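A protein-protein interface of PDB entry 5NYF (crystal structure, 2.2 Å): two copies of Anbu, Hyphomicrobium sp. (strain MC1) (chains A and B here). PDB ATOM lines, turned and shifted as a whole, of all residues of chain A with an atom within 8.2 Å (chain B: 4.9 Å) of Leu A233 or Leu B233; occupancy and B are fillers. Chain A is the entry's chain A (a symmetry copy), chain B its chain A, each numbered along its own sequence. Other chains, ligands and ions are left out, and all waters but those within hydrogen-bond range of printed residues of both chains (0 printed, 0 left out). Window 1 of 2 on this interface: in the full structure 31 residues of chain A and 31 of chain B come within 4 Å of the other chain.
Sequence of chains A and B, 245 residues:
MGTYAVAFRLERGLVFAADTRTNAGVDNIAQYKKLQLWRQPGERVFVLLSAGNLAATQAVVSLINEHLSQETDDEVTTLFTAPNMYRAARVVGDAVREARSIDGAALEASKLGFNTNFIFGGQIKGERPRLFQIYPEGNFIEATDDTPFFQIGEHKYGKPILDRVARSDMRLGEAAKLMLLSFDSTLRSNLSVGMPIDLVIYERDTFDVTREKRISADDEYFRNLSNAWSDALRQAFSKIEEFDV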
ATOM      1  N   PRO A 160      -2.309  16.048 -16.558  1.00  0.00           N
ATOM      2  CA  PRO A 160      -1.355  16.857 -15.789  1.00  0.00           C
ATOM      3  C   PRO A 160      -1.329  18.350 -16.144  1.00  0.00           C
ATOM      4  O   PRO A 160      -1.181  19.172 -15.241  1.00  0.00           O
ATOM      5  CB  PRO A 160       0.007  16.201 -16.091  1.00  0.00           C
ATOM      6  CG  PRO A 160      -0.232  15.237 -17.203  1.00  0.00           C
ATOM      7  CD  PRO A 160      -1.661  14.825 -17.067  1.00  0.00           C
ATOM      8  N   ILE A 161      -1.471  18.687 -17.427  1.00  0.00           N
ATOM      9  CA  ILE A 161      -1.536  20.093 -17.855  1.00  0.00           C
ATOM     10  C   ILE A 161      -2.814  20.766 -17.343  1.00  0.00           C
ATOM     11  O   ILE A 161      -2.758  21.877 -16.800  1.00  0.00           O
ATOM     12  CB  ILE A 161      -1.436  20.245 -19.394  1.00  0.00           C
ATOM     13  CG1 ILE A 161      -0.044  19.827 -19.873  1.00  0.00           C
ATOM     14  CG2 ILE A 161      -1.716  21.687 -19.828  1.00  0.00           C
ATOM     15  CD1 ILE A 161       0.043  19.549 -21.361  1.00  0.00           C
ATOM     16  N   LEU A 162      -3.956  20.097 -17.518  1.00  0.00           N
ATOM     17  CA  LEU A 162      -5.239  20.634 -17.062  1.00  0.00           C
ATOM     18  C   LEU A 162      -5.254  20.867 -15.550  1.00  0.00           C
ATOM     19  O   LEU A 162      -5.683  21.922 -15.097  1.00  0.00           O
ATOM     20  CB  LEU A 162      -6.397  19.716 -17.466  1.00  0.00           C
ATOM     21  CG  LEU A 162      -6.666  19.500 -18.963  1.00  0.00           C
ATOM     22  CD1 LEU A 162      -7.868  18.586 -19.152  1.00  0.00           C
ATOM     23  CD2 LEU A 162      -6.887  20.813 -19.692  1.00  0.00           C
ATOM     24  N   ASP A 163      -4.759  19.891 -14.784  1.00  0.00           N
ATOM     25  CA  ASP A 163      -4.648  20.008 -13.316  1.00  0.00           C
ATOM     26  C   ASP A 163      -3.880  21.255 -12.876  1.00  0.00           C
ATOM     27  O   ASP A 163      -4.251  21.906 -11.898  1.00  0.00           O
ATOM     28  CB  ASP A 163      -3.940  18.778 -12.714  1.00  0.00           C
ATOM     29  CG  ASP A 163      -4.789  17.514 -12.753  1.00  0.00           C
ATOM     30  OD1 ASP A 163      -6.025  17.595 -12.604  1.00  0.00           O
ATOM     31  OD2 ASP A 163      -4.205  16.419 -12.914  1.00  0.00           O
ATOM     32  N   ARG A 164      -2.811  21.569 -13.600  1.00  0.00           N
ATOM     33  CA  ARG A 164      -1.902  22.658 -13.232  1.00  0.00           C
ATOM     34  C   ARG A 164      -2.364  24.037 -13.727  1.00  0.00           C
ATOM     35  O   ARG A 164      -2.133  25.042 -13.046  1.00  0.00           O
ATOM     36  CB  ARG A 164      -0.490  22.358 -13.754  1.00  0.00           C
ATOM     37  CG  ARG A 164       0.162  21.136 -13.106  1.00  0.00           C
ATOM     38  CD  ARG A 164       1.419  20.722 -13.860  1.00  0.00           C
ATOM     39  NE  ARG A 164       2.049  19.508 -13.328  1.00  0.00           N
ATOM     40  CZ  ARG A 164       3.003  19.456 -12.388  1.00  0.00           C
ATOM     41  NH1 ARG A 164       3.489  20.555 -11.805  1.00  0.00           N
ATOM     42  NH2 ARG A 164       3.480  18.271 -12.019  1.00  0.00           N
ATOM     43  N   VAL A 165      -3.015  24.079 -14.891  1.00  0.00           N
ATOM     44  CA  VAL A 165      -3.356  25.345 -15.563  1.00  0.00           C
ATOM     45  C   VAL A 165      -4.837  25.755 -15.429  1.00  0.00           C
ATOM     46  O   VAL A 165      -5.128  26.942 -15.321  1.00  0.00           O
ATOM     47  CB  VAL A 165      -2.928  25.302 -17.050  1.00  0.00           C
ATOM     48  CG1 VAL A 165      -3.254  26.610 -17.764  1.00  0.00           C
ATOM     49  CG2 VAL A 165      -1.433  25.013 -17.152  1.00  0.00           C
ATOM     50  N   LEU A 178      -7.519  25.794 -23.863  1.00  0.00           N
ATOM     51  CA  LEU A 178      -6.840  24.833 -22.994  1.00  0.00           C
ATOM     52  C   LEU A 178      -7.329  23.406 -23.241  1.00  0.00           C
ATOM     53  O   LEU A 178      -6.521  22.475 -23.346  1.00  0.00           O
ATOM     54  CB  LEU A 178      -7.039  25.198 -21.519  1.00  0.00           C
ATOM     55  CG  LEU A 178      -6.352  24.307 -20.479  1.00  0.00           C
ATOM     56  CD1 LEU A 178      -4.843  24.279 -20.679  1.00  0.00           C
ATOM     57  CD2 LEU A 178      -6.699  24.770 -19.070  1.00  0.00           C
ATOM     58  N   LEU A 181      -6.084  22.000 -26.616  1.00  0.00           N
ATOM     59  CA  LEU A 181      -4.685  21.561 -26.558  1.00  0.00           C
ATOM     60  C   LEU A 181      -4.526  20.178 -25.919  1.00  0.00           C
ATOM     61  O   LEU A 181      -3.594  19.451 -26.258  1.00  0.00           O
ATOM     62  CB  LEU A 181      -3.816  22.594 -25.837  1.00  0.00           C
ATOM     63  CG  LEU A 181      -3.648  23.910 -26.608  1.00  0.00           C
ATOM     64  CD1 LEU A 181      -3.149  25.022 -25.696  1.00  0.00           C
ATOM     65  CD2 LEU A 181      -2.722  23.739 -27.807  1.00  0.00           C
ATOM     66  N   SER A 226      -1.445  25.185 -31.578  1.00  0.00           N
ATOM     67  CA  SER A 226      -0.654  24.011 -31.191  1.00  0.00           C
ATOM     68  C   SER A 226       0.849  24.235 -31.361  1.00  0.00           C
ATOM     69  O   SER A 226       1.624  23.831 -30.494  1.00  0.00           O
ATOM     70  CB  SER A 226      -1.090  22.773 -31.977  1.00  0.00           C
ATOM     71  OG  SER A 226      -0.408  21.616 -31.519  1.00  0.00           O
ATOM     72  N   ASN A 227       1.247  24.875 -32.464  1.00  0.00           N
ATOM     73  CA  ASN A 227       2.661  25.226 -32.700  1.00  0.00           C
ATOM     74  C   ASN A 227       3.194  26.214 -31.666  1.00  0.00           C
ATOM     75  O   ASN A 227       4.322  26.070 -31.187  1.00  0.00           O
ATOM     76  CB  ASN A 227       2.868  25.822 -34.105  1.00  0.00           C
ATOM     77  CG  ASN A 227       2.715  24.797 -35.219  1.00  0.00           C
ATOM     78  OD1 ASN A 227       2.938  23.599 -35.030  1.00  0.00           O
ATOM     79  ND2 ASN A 227       2.342  25.276 -36.401  1.00  0.00           N
ATOM     80  N   ALA A 228       2.388  27.220 -31.343  1.00  0.00           N
ATOM     81  CA  ALA A 228       2.756  28.213 -30.334  1.00  0.00           C
ATOM     82  C   ALA A 228       2.884  27.580 -28.946  1.00  0.00           C
ATOM     83  O   ALA A 228       3.768  27.960 -28.173  1.00  0.00           O
ATOM     84  CB  ALA A 228       1.744  29.353 -30.309  1.00  0.00           C
ATOM     85  N   TRP A 229       1.997  26.628 -28.643  1.00  0.00           N
ATOM     86  CA  TRP A 229       2.034  25.880 -27.384  1.00  0.00           C
ATOM     87  C   TRP A 229       3.330  25.072 -27.242  1.00  0.00           C
ATOM     88  O   TRP A 229       3.958  25.094 -26.180  1.00  0.00           O
ATOM     89  CB  TRP A 229       0.798  24.976 -27.279  1.00  0.00           C
ATOM     90  CG  TRP A 229       0.678  24.151 -26.023  1.00  0.00           C
ATOM     91  CD1 TRP A 229       0.477  22.800 -25.955  1.00  0.00           C
ATOM     92  CD2 TRP A 229       0.730  24.615 -24.668  1.00  0.00           C
ATOM     93  NE1 TRP A 229       0.403  22.398 -24.648  1.00  0.00           N
ATOM     94  CE2 TRP A 229       0.558  23.489 -23.835  1.00  0.00           C
ATOM     95  CE3 TRP A 229       0.906  25.872 -24.075  1.00  0.00           C
ATOM     96  CZ2 TRP A 229       0.557  23.581 -22.437  1.00  0.00           C
ATOM     97  CZ3 TRP A 229       0.908  25.963 -22.678  1.00  0.00           C
ATOM     98  CH2 TRP A 229       0.734  24.824 -21.881  1.00  0.00           C
ATOM     99  N   SER A 230       3.733  24.384 -28.311  1.00  0.00           N
ATOM    100  CA  SER A 230       5.014  23.660 -28.336  1.00  0.00           C
ATOM    101  C   SER A 230       6.198  24.583 -28.067  1.00  0.00           C
ATOM    102  O   SER A 230       7.073  24.247 -27.273  1.00  0.00           O
ATOM    103  CB  SER A 230       5.221  22.942 -29.671  1.00  0.00           C
ATOM    104  OG  SER A 230       4.319  21.862 -29.802  1.00  0.00           O
ATOM    105  N   ASP A 231       6.209  25.743 -28.720  1.00  0.00           N
ATOM    106  CA  ASP A 231       7.251  26.750 -28.500  1.00  0.00           C
ATOM    107  C   ASP A 231       7.245  27.281 -27.068  1.00  0.00           C
ATOM    108  O   ASP A 231       8.304  27.479 -26.477  1.00  0.00           O
ATOM    109  CB  ASP A 231       7.095  27.923 -29.480  1.00  0.00           C
ATOM    110  CG  ASP A 231       7.372  27.530 -30.925  1.00  0.00           C
ATOM    111  OD1 ASP A 231       7.788  26.376 -31.178  1.00  0.00           O
ATOM    112  OD2 ASP A 231       7.170  28.382 -31.817  1.00  0.00           O
ATOM    113  N   ALA A 232       6.052  27.505 -26.523  1.00  0.00           N
ATOM    114  CA  ALA A 232       5.903  27.983 -25.150  1.00  0.00           C
ATOM    115  C   ALA A 232       6.302  26.926 -24.117  1.00  0.00           C
ATOM    116  O   ALA A 232       6.869  27.266 -23.076  1.00  0.00           O
ATOM    117  CB  ALA A 232       4.476  28.453 -24.905  1.00  0.00           C
ATOM    118  N   LEU A 233       6.005  25.658 -24.396  1.00  0.00           N
ATOM    119  CA  LEU A 233       6.435  24.557 -23.523  1.00  0.00           C
ATOM    120  C   LEU A 233       7.957  24.436 -23.438  1.00  0.00           C
ATOM    121  O   LEU A 233       8.502  24.265 -22.341  1.00  0.00           O
ATOM    122  CB  LEU A 233       5.828  23.221 -23.961  1.00  0.00           C
ATOM    123  CG  LEU A 233       4.344  23.025 -23.638  1.00  0.00           C
ATOM    124  CD1 LEU A 233       3.831  21.783 -24.347  1.00  0.00           C
ATOM    125  CD2 LEU A 233       4.096  22.928 -22.137  1.00  0.00           C
ATOM    126  N   ARG A 234       8.633  24.530 -24.585  1.00  0.00           N
ATOM    127  CA  ARG A 234      10.098  24.475 -24.634  1.00  0.00           C
ATOM    128  C   ARG A 234      10.727  25.623 -23.859  1.00  0.00           C
ATOM    129  O   ARG A 234      11.686  25.416 -23.131  1.00  0.00           O
ATOM    130  CB  ARG A 234      10.615  24.496 -26.071  1.00  0.00           C
ATOM    131  CG  ARG A 234      10.287  23.251 -26.867  1.00  0.00           C
ATOM    132  CD  ARG A 234      10.955  23.257 -28.231  1.00  0.00           C
ATOM    133  NE  ARG A 234      10.026  22.843 -29.289  1.00  0.00           N
ATOM    134  CZ  ARG A 234       9.586  23.601 -30.303  1.00  0.00           C
ATOM    135  NH1 ARG A 234       8.742  23.074 -31.188  1.00  0.00           N
ATOM    136  NH2 ARG A 234       9.972  24.870 -30.467  1.00  0.00           N
ATOM    137  N   GLN A 235      10.185  26.827 -24.022  1.00  0.00           N
ATOM    138  CA  GLN A 235      10.643  27.990 -23.257  1.00  0.00           C
ATOM    139  C   GLN A 235      10.357  27.845 -21.759  1.00  0.00           C
ATOM    140  O   GLN A 235      11.192  28.206 -20.936  1.00  0.00           O
ATOM    141  CB  GLN A 235      10.028  29.291 -23.800  1.00  0.00           C
ATOM    142  CG  GLN A 235      10.554  29.703 -25.171  1.00  0.00           C
ATOM    143  CD  GLN A 235      12.024  30.118 -25.153  1.00  0.00           C
ATOM    144  OE1 GLN A 235      12.858  29.530 -25.848  1.00  0.00           O
ATOM    145  NE2 GLN A 235      12.346  31.129 -24.350  1.00  0.00           N
ATOM    146  N   ALA A 236       9.183  27.319 -21.414  1.00  0.00           N
ATOM    147  CA  ALA A 236       8.836  27.055 -20.012  1.00  0.00           C
ATOM    148  C   ALA A 236       9.809  26.065 -19.374  1.00  0.00           C
ATOM    149  O   ALA A 236      10.242  26.263 -18.233  1.00  0.00           O
ATOM    150  CB  ALA A 236       7.410  26.535 -19.903  1.00  0.00           C
ATOM    151  N   PHE A 237      10.158  25.010 -20.114  1.00  0.00           N
ATOM    152  CA  PHE A 237      11.121  24.026 -19.626  1.00  0.00           C
ATOM    153  C   PHE A 237      12.527  24.615 -19.503  1.00  0.00           C
ATOM    154  O   PHE A 237      13.211  24.355 -18.521  1.00  0.00           O
ATOM    155  CB  PHE A 237      11.156  22.772 -20.495  1.00  0.00           C
ATOM    156  CG  PHE A 237      12.036  21.697 -19.934  1.00  0.00           C
ATOM    157  CD1 PHE A 237      11.644  20.997 -18.804  1.00  0.00           C
ATOM    158  CD2 PHE A 237      13.278  21.422 -20.495  1.00  0.00           C
ATOM    159  CE1 PHE A 237      12.454  20.022 -18.261  1.00  0.00           C
ATOM    160  CE2 PHE A 237      14.095  20.448 -19.958  1.00  0.00           C
ATOM    161  CZ  PHE A 237      13.681  19.745 -18.839  1.00  0.00           C
ATOM    162  N   SER A 238      12.953  25.398 -20.494  1.00  0.00           N
ATOM    163  CA  SER A 238      14.243  26.103 -20.423  1.00  0.00           C
ATOM    164  C   SER A 238      14.403  26.937 -19.153  1.00  0.00           C
ATOM    165  O   SER A 238      15.488  26.980 -18.581  1.00  0.00           O
ATOM    166  CB  SER A 238      14.456  26.996 -21.647  1.00  0.00           C
ATOM    167  OG  SER A 238      14.881  26.222 -22.749  1.00  0.00           O
ATOM    168  N   LYS A 239      13.326  27.589 -18.721  1.00  0.00           N
ATOM    169  CA  LYS A 239      13.339  28.388 -17.490  1.00  0.00           C
ATOM    170  C   LYS A 239      13.554  27.514 -16.259  1.00  0.00           C
ATOM    171  O   LYS A 239      14.473  27.755 -15.479  1.00  0.00           O
ATOM    172  CB  LYS A 239      12.037  29.184 -17.340  1.00  0.00           C
ATOM    173  CG  LYS A 239      11.860  30.293 -18.366  1.00  0.00           C
ATOM    174  CD  LYS A 239      12.579  31.570 -17.952  1.00  0.00           C
ATOM    175  CE  LYS A 239      12.364  32.689 -18.962  1.00  0.00           C
ATOM    176  NZ  LYS A 239      12.532  34.032 -18.339  1.00  0.00           N
ATOM    177  N   ILE A 240      12.713  26.493 -16.109  1.00  0.00           N
ATOM    178  CA  ILE A 240      12.742  25.625 -14.920  1.00  0.00           C
ATOM    179  C   ILE A 240      13.923  24.652 -14.849  1.00  0.00           C
ATOM    180  O   ILE A 240      14.117  24.020 -13.814  1.00  0.00           O
ATOM    181  CB  ILE A 240      11.403  24.870 -14.693  1.00  0.00           C
ATOM    182  CG1 ILE A 240      11.110  23.846 -15.798  1.00  0.00           C
ATOM    183  CG2 ILE A 240      10.258  25.865 -14.555  1.00  0.00           C
ATOM    184  CD1 ILE A 240      11.617  22.445 -15.534  1.00  0.00           C
ATOM    185  N   ILE B 161       3.673  16.305 -23.630  1.00  0.00           N
ATOM    186  CA  ILE B 161       4.780  17.177 -23.211  1.00  0.00           C
ATOM    187  C   ILE B 161       6.124  16.644 -23.725  1.00  0.00           C
ATOM    188  O   ILE B 161       6.927  17.408 -24.275  1.00  0.00           O
ATOM    189  CB  ILE B 161       4.835  17.361 -21.674  1.00  0.00           C
ATOM    190  CG1 ILE B 161       3.611  18.147 -21.197  1.00  0.00           C
ATOM    191  CG2 ILE B 161       6.111  18.094 -21.250  1.00  0.00           C
ATOM    192  CD1 ILE B 161       3.348  18.042 -19.707  1.00  0.00           C
ATOM    193  N   ARG B 164       6.718  17.145 -27.473  1.00  0.00           N
ATOM    194  CA  ARG B 164       6.948  18.542 -27.851  1.00  0.00           C
ATOM    195  C   ARG B 164       8.295  19.096 -27.365  1.00  0.00           C
ATOM    196  O   ARG B 164       8.904  19.922 -28.053  1.00  0.00           O
ATOM    197  CB  ARG B 164       5.800  19.420 -27.332  1.00  0.00           C
ATOM    198  CG  ARG B 164       4.448  19.112 -27.973  1.00  0.00           C
ATOM    199  CD  ARG B 164       3.316  19.799 -27.221  1.00  0.00           C
ATOM    200  NE  ARG B 164       1.983  19.479 -27.746  1.00  0.00           N
ATOM    201  CZ  ARG B 164       1.318  20.161 -28.688  1.00  0.00           C
ATOM    202  NH1 ARG B 164       1.830  21.242 -29.281  1.00  0.00           N
ATOM    203  NH2 ARG B 164       0.107  19.746 -29.051  1.00  0.00           N
ATOM    204  N   VAL B 165       8.756  18.638 -26.198  1.00  0.00           N
ATOM    205  CA  VAL B 165       9.940  19.211 -25.534  1.00  0.00           C
ATOM    206  C   VAL B 165      11.217  18.356 -25.666  1.00  0.00           C
ATOM    207  O   VAL B 165      12.305  18.910 -25.782  1.00  0.00           O
ATOM    208  CB  VAL B 165       9.632  19.517 -24.048  1.00  0.00           C
ATOM    209  CG1 VAL B 165      10.838  20.130 -23.342  1.00  0.00           C
ATOM    210  CG2 VAL B 165       8.438  20.462 -23.949  1.00  0.00           C
ATOM    211  N   TRP B 229       7.457  24.193 -12.480  1.00  0.00           N
ATOM    212  CA  TRP B 229       6.862  23.724 -13.734  1.00  0.00           C
ATOM    213  C   TRP B 229       5.404  24.177 -13.874  1.00  0.00           C
ATOM    214  O   TRP B 229       5.008  24.660 -14.938  1.00  0.00           O
ATOM    215  CB  TRP B 229       6.985  22.197 -13.829  1.00  0.00           C
ATOM    216  CG  TRP B 229       6.434  21.558 -15.079  1.00  0.00           C
ATOM    217  CD1 TRP B 229       5.542  20.524 -15.137  1.00  0.00           C
ATOM    218  CD2 TRP B 229       6.748  21.892 -16.437  1.00  0.00           C
ATOM    219  NE1 TRP B 229       5.281  20.196 -16.441  1.00  0.00           N
ATOM    220  CE2 TRP B 229       6.004  21.021 -17.262  1.00  0.00           C
ATOM    221  CE3 TRP B 229       7.583  22.842 -17.040  1.00  0.00           C
ATOM    222  CZ2 TRP B 229       6.071  21.070 -18.661  1.00  0.00           C
ATOM    223  CZ3 TRP B 229       7.645  22.893 -18.436  1.00  0.00           C
ATOM    224  CH2 TRP B 229       6.895  22.012 -19.226  1.00  0.00           C
ATOM    225  N   SER B 230       4.624  24.040 -12.802  1.00  0.00           N
ATOM    226  CA  SER B 230       3.239  24.538 -12.777  1.00  0.00           C
ATOM    227  C   SER B 230       3.164  26.036 -13.056  1.00  0.00           C
ATOM    228  O   SER B 230       2.335  26.474 -13.850  1.00  0.00           O
ATOM    229  CB  SER B 230       2.564  24.235 -11.437  1.00  0.00           C
ATOM    230  OG  SER B 230       2.335  22.848 -11.295  1.00  0.00           O
ATOM    231  N   ASP B 231       4.038  26.806 -12.410  1.00  0.00           N
ATOM    232  CA  ASP B 231       4.119  28.251 -12.640  1.00  0.00           C
ATOM    233  C   ASP B 231       4.520  28.583 -14.075  1.00  0.00           C
ATOM    234  O   ASP B 231       3.977  29.511 -14.672  1.00  0.00           O
ATOM    235  CB  ASP B 231       5.112  28.906 -11.668  1.00  0.00           C
ATOM    236  CG  ASP B 231       4.638  28.868 -10.221  1.00  0.00           C
ATOM    237  OD1 ASP B 231       3.494  28.432  -9.961  1.00  0.00           O
ATOM    238  OD2 ASP B 231       5.418  29.278  -9.334  1.00  0.00           O
ATOM    239  N   ALA B 232       5.467  27.823 -14.619  1.00  0.00           N
ATOM    240  CA  ALA B 232       5.922  28.012 -15.995  1.00  0.00           C
ATOM    241  C   ALA B 232       4.858  27.617 -17.021  1.00  0.00           C
ATOM    242  O   ALA B 232       4.742  28.261 -18.066  1.00  0.00           O
ATOM    243  CB  ALA B 232       7.210  27.237 -16.238  1.00  0.00           C
ATOM    244  N   LEU B 233       4.092  26.566 -16.733  1.00  0.00           N
ATOM    245  CA  LEU B 233       2.974  26.167 -17.600  1.00  0.00           C
ATOM    246  C   LEU B 233       1.889  27.240 -17.689  1.00  0.00           C
ATOM    247  O   LEU B 233       1.400  27.534 -18.786  1.00  0.00           O
ATOM    248  CB  LEU B 233       2.361  24.838 -17.151  1.00  0.00           C
ATOM    249  CG  LEU B 233       3.180  23.584 -17.467  1.00  0.00           C
ATOM    250  CD1 LEU B 233       2.577  22.389 -16.749  1.00  0.00           C
ATOM    251  CD2 LEU B 233       3.263  23.323 -18.967  1.00  0.00           C
ATOM    252  N   ARG B 234       1.523  27.821 -16.545  1.00  0.00           N
ATOM    253  CA  ARG B 234       0.525  28.896 -16.500  1.00  0.00           C
ATOM    254  C   ARG B 234       0.981  30.116 -17.284  1.00  0.00           C
ATOM    255  O   ARG B 234       0.195  30.701 -18.013  1.00  0.00           O
ATOM    256  CB  ARG B 234       0.208  29.311 -15.064  1.00  0.00           C
ATOM    257  CG  ARG B 234      -0.519  28.254 -14.259  1.00  0.00           C
ATOM    258  CD  ARG B 234      -0.946  28.774 -12.897  1.00  0.00           C
ATOM    259  NE  ARG B 234      -0.650  27.807 -11.833  1.00  0.00           N
ATOM    260  CZ  ARG B 234       0.215  27.976 -10.823  1.00  0.00           C
ATOM    261  NH1 ARG B 234       0.369  26.998  -9.932  1.00  0.00           N
ATOM    262  NH2 ARG B 234       0.924  29.098 -10.669  1.00  0.00           N
ATOM    263  N   GLN B 235       2.248  30.492 -17.128  1.00  0.00           N
ATOM    264  CA  GLN B 235       2.826  31.594 -17.902  1.00  0.00           C
ATOM    265  C   GLN B 235       2.900  31.272 -19.398  1.00  0.00           C
ATOM    266  O   GLN B 235       2.624  32.135 -20.226  1.00  0.00           O
ATOM    267  CB  GLN B 235       4.214  31.981 -17.367  1.00  0.00           C
ATOM    268  CG  GLN B 235       4.188  32.658 -16.000  1.00  0.00           C
ATOM    269  CD  GLN B 235       3.543  34.042 -16.026  1.00  0.00           C
ATOM    270  OE1 GLN B 235       2.555  34.295 -15.329  1.00  0.00           O
ATOM    271  NE2 GLN B 235       4.096  34.940 -16.836  1.00  0.00           N
ATOM    272  N   ALA B 236       3.266  30.038 -19.736  1.00  0.00           N
ATOM    273  CA  ALA B 236       3.289  29.593 -21.135  1.00  0.00           C
ATOM    274  C   ALA B 236       1.901  29.679 -21.770  1.00  0.00           C
ATOM    275  O   ALA B 236       1.765  30.128 -22.913  1.00  0.00           O
ATOM    276  CB  ALA B 236       3.825  28.171 -21.236  1.00  0.00           C
ATOM    277  N   PHE B 237       0.877  29.259 -21.023  1.00  0.00           N
ATOM    278  CA  PHE B 237      -0.499  29.343 -21.508  1.00  0.00           C
ATOM    279  C   PHE B 237      -0.972  30.791 -21.639  1.00  0.00           C
ATOM    280  O   PHE B 237      -1.618  31.132 -22.621  1.00  0.00           O
ATOM    281  CB  PHE B 237      -1.469  28.556 -20.630  1.00  0.00           C
ATOM    282  CG  PHE B 237      -2.859  28.517 -21.187  1.00  0.00           C
ATOM    283  CD1 PHE B 237      -3.138  27.755 -22.311  1.00  0.00           C
ATOM    284  CD2 PHE B 237      -3.876  29.282 -20.628  1.00  0.00           C
ATOM    285  CE1 PHE B 237      -4.406  27.729 -22.849  1.00  0.00           C
ATOM    286  CE2 PHE B 237      -5.150  29.261 -21.161  1.00  0.00           C
ATOM    287  CZ  PHE B 237      -5.415  28.481 -22.273  1.00  0.00           C
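NE of Arg B234 sits at hydrogen-bond distance from O of Arg A164 (3.4 Å). The guanidinium group (NE) of Arg A234 is in hydrogen-bond range of the backbone carbonyl oxygen (O) of Arg B164, at 3.4 Å. NH1 of Arg B164 lies within hydrogen-bond range of O of Ser A226 (2.9 Å). The side-chain hydroxyl (OG) of Ser A230 lies within hydrogen-bond range of the guanidinium group (NH1) of Arg B164. The guanidinium group (NH1) of Arg A164 sits at hydrogen-bond distance from the side-chain hydroxyl (OG) of Ser B230 (2.6 Å).
Arg A164 touches Leu B233, and with the chains exchanged Leu A233 touches Arg B164. Arg A164 touches Arg B234, and with the chains exchanged Arg A234 touches Arg B164. Val A165 touches Phe B237, and with the chains exchanged Phe A237 touches Val B165. Leu B233 touches its own counterpart, Leu A233. Of the 24 pairs that touch across the chains among the printed residues, 20 have their exchanged pair printed and touching as well.
Leu A233 touches just these residues of chain B: Arg B164, Val B165 and Leu B233. Leu B233 touches three residues of chain A. Of chain A, only Ala A236 and Ile A240 come within 4 Å of Ala B232. Printed residues of chain B within 4 Å of Ile A240: Trp B229 (3.9 Å) and Ala B232 (3.7 Å). Of the printed residues of chain A, Ser B230 touches Arg A164. Printed residues of chain B within 4 Å of Arg A164: Trp B229 (3.9 Å), Ser B230 (2.6 Å), Leu B233 (3.5 Å) and Arg B234 (3.4 Å). Of the printed residues of chain A, Arg B164 touches Ser A226 (2.9 Å), Trp A229 (3.9 Å), Ser A230 (2.6 Å), Leu A233 (3.5 Å) and Arg A234 (3.4 Å). The nearest printed residue of chain B that does not touch Ser A230 is Val B165 (5.2 Å).
Among the printed residues, merely in contact across the chains: Leu A233 with Leu B233 (3.3 Å), Leu A233 with Arg B164 (3.5 Å), Arg A164 with Leu B233 (3.5 Å), Ala A232 with Ala B236 (3.7 Å), Ala A236 with Ala B232 (3.7 Å), Trp A229 with Phe B237 (3.7 Å), Phe A237 with Trp B229 (3.7 Å), Leu A178 with Phe B237 (3.7 Å), Ile A240 with Ala B232 (3.7 Å), Leu A233 with Val B165 (3.8 Å), Val A165 with Leu B233 (3.8 Å), Ile A161 with Ile B161 (3.8 Å), Ile A240 with Trp B229 (3.9 Å), Trp A229 with Arg B164 (3.9 Å), Arg A164 with Trp B229 (3.9 Å), Phe A237 with Val B165 (3.9 Å), Val A165 with Phe B237 (3.9 Å), Trp A229 with Ala B236 (3.9 Å) and Ala A236 with Trp B229 (3.9 Å).
The backbone carbonyl oxygen (O) of Ser A226 is in hydrogen-bond range of the side-chain hydroxyl (OG) of Ser A230, 3.4 Å away. OD1 of Asp B231 lies within salt-bridge range of NH2 of Arg B234 (2.7 Å). The guanidinium group (NH2) of Arg A234 lies within salt-bridge range of the side-chain carboxylate (OD1) of Asp A231 (2.7 Å). The side-chain hydroxyl of Ser A238 lies within hydrogen-bond range of the backbone carbonyl oxygen of Arg A234 (3.3 Å).
Of the 23 printed residues of chain A, 13 touch a printed residue of chain B. Printed residues of chain A that touch a printed residue of chain B: Ile A161, Arg A164, Val A165, Leu A178, Ser A226, Trp A229, Ser A230, Ala A232, Leu A233, Arg A234, Ala A236, Phe A237 and Ile A240. Hydrophobic or aromatic side chains of chain A within 4 Å of the printed part of chain B: Ile A161, Val A165, Leu A178, Trp A229, Ala A232, Leu A233, Ala A236, Phe A237 and Ile A240. Along chain A the printed residues that touch a printed residue of chain B span positions 161 to 240. Of the 12 printed residues of chain B, 10 touch a printed residue of chain A. Among the printed residues, 24 pairs touch across the chains. Among the printed residues, no Asp or Glu carboxylate lies within 4 Å of a Lys or Arg side-chain nitrogen of the other chain.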
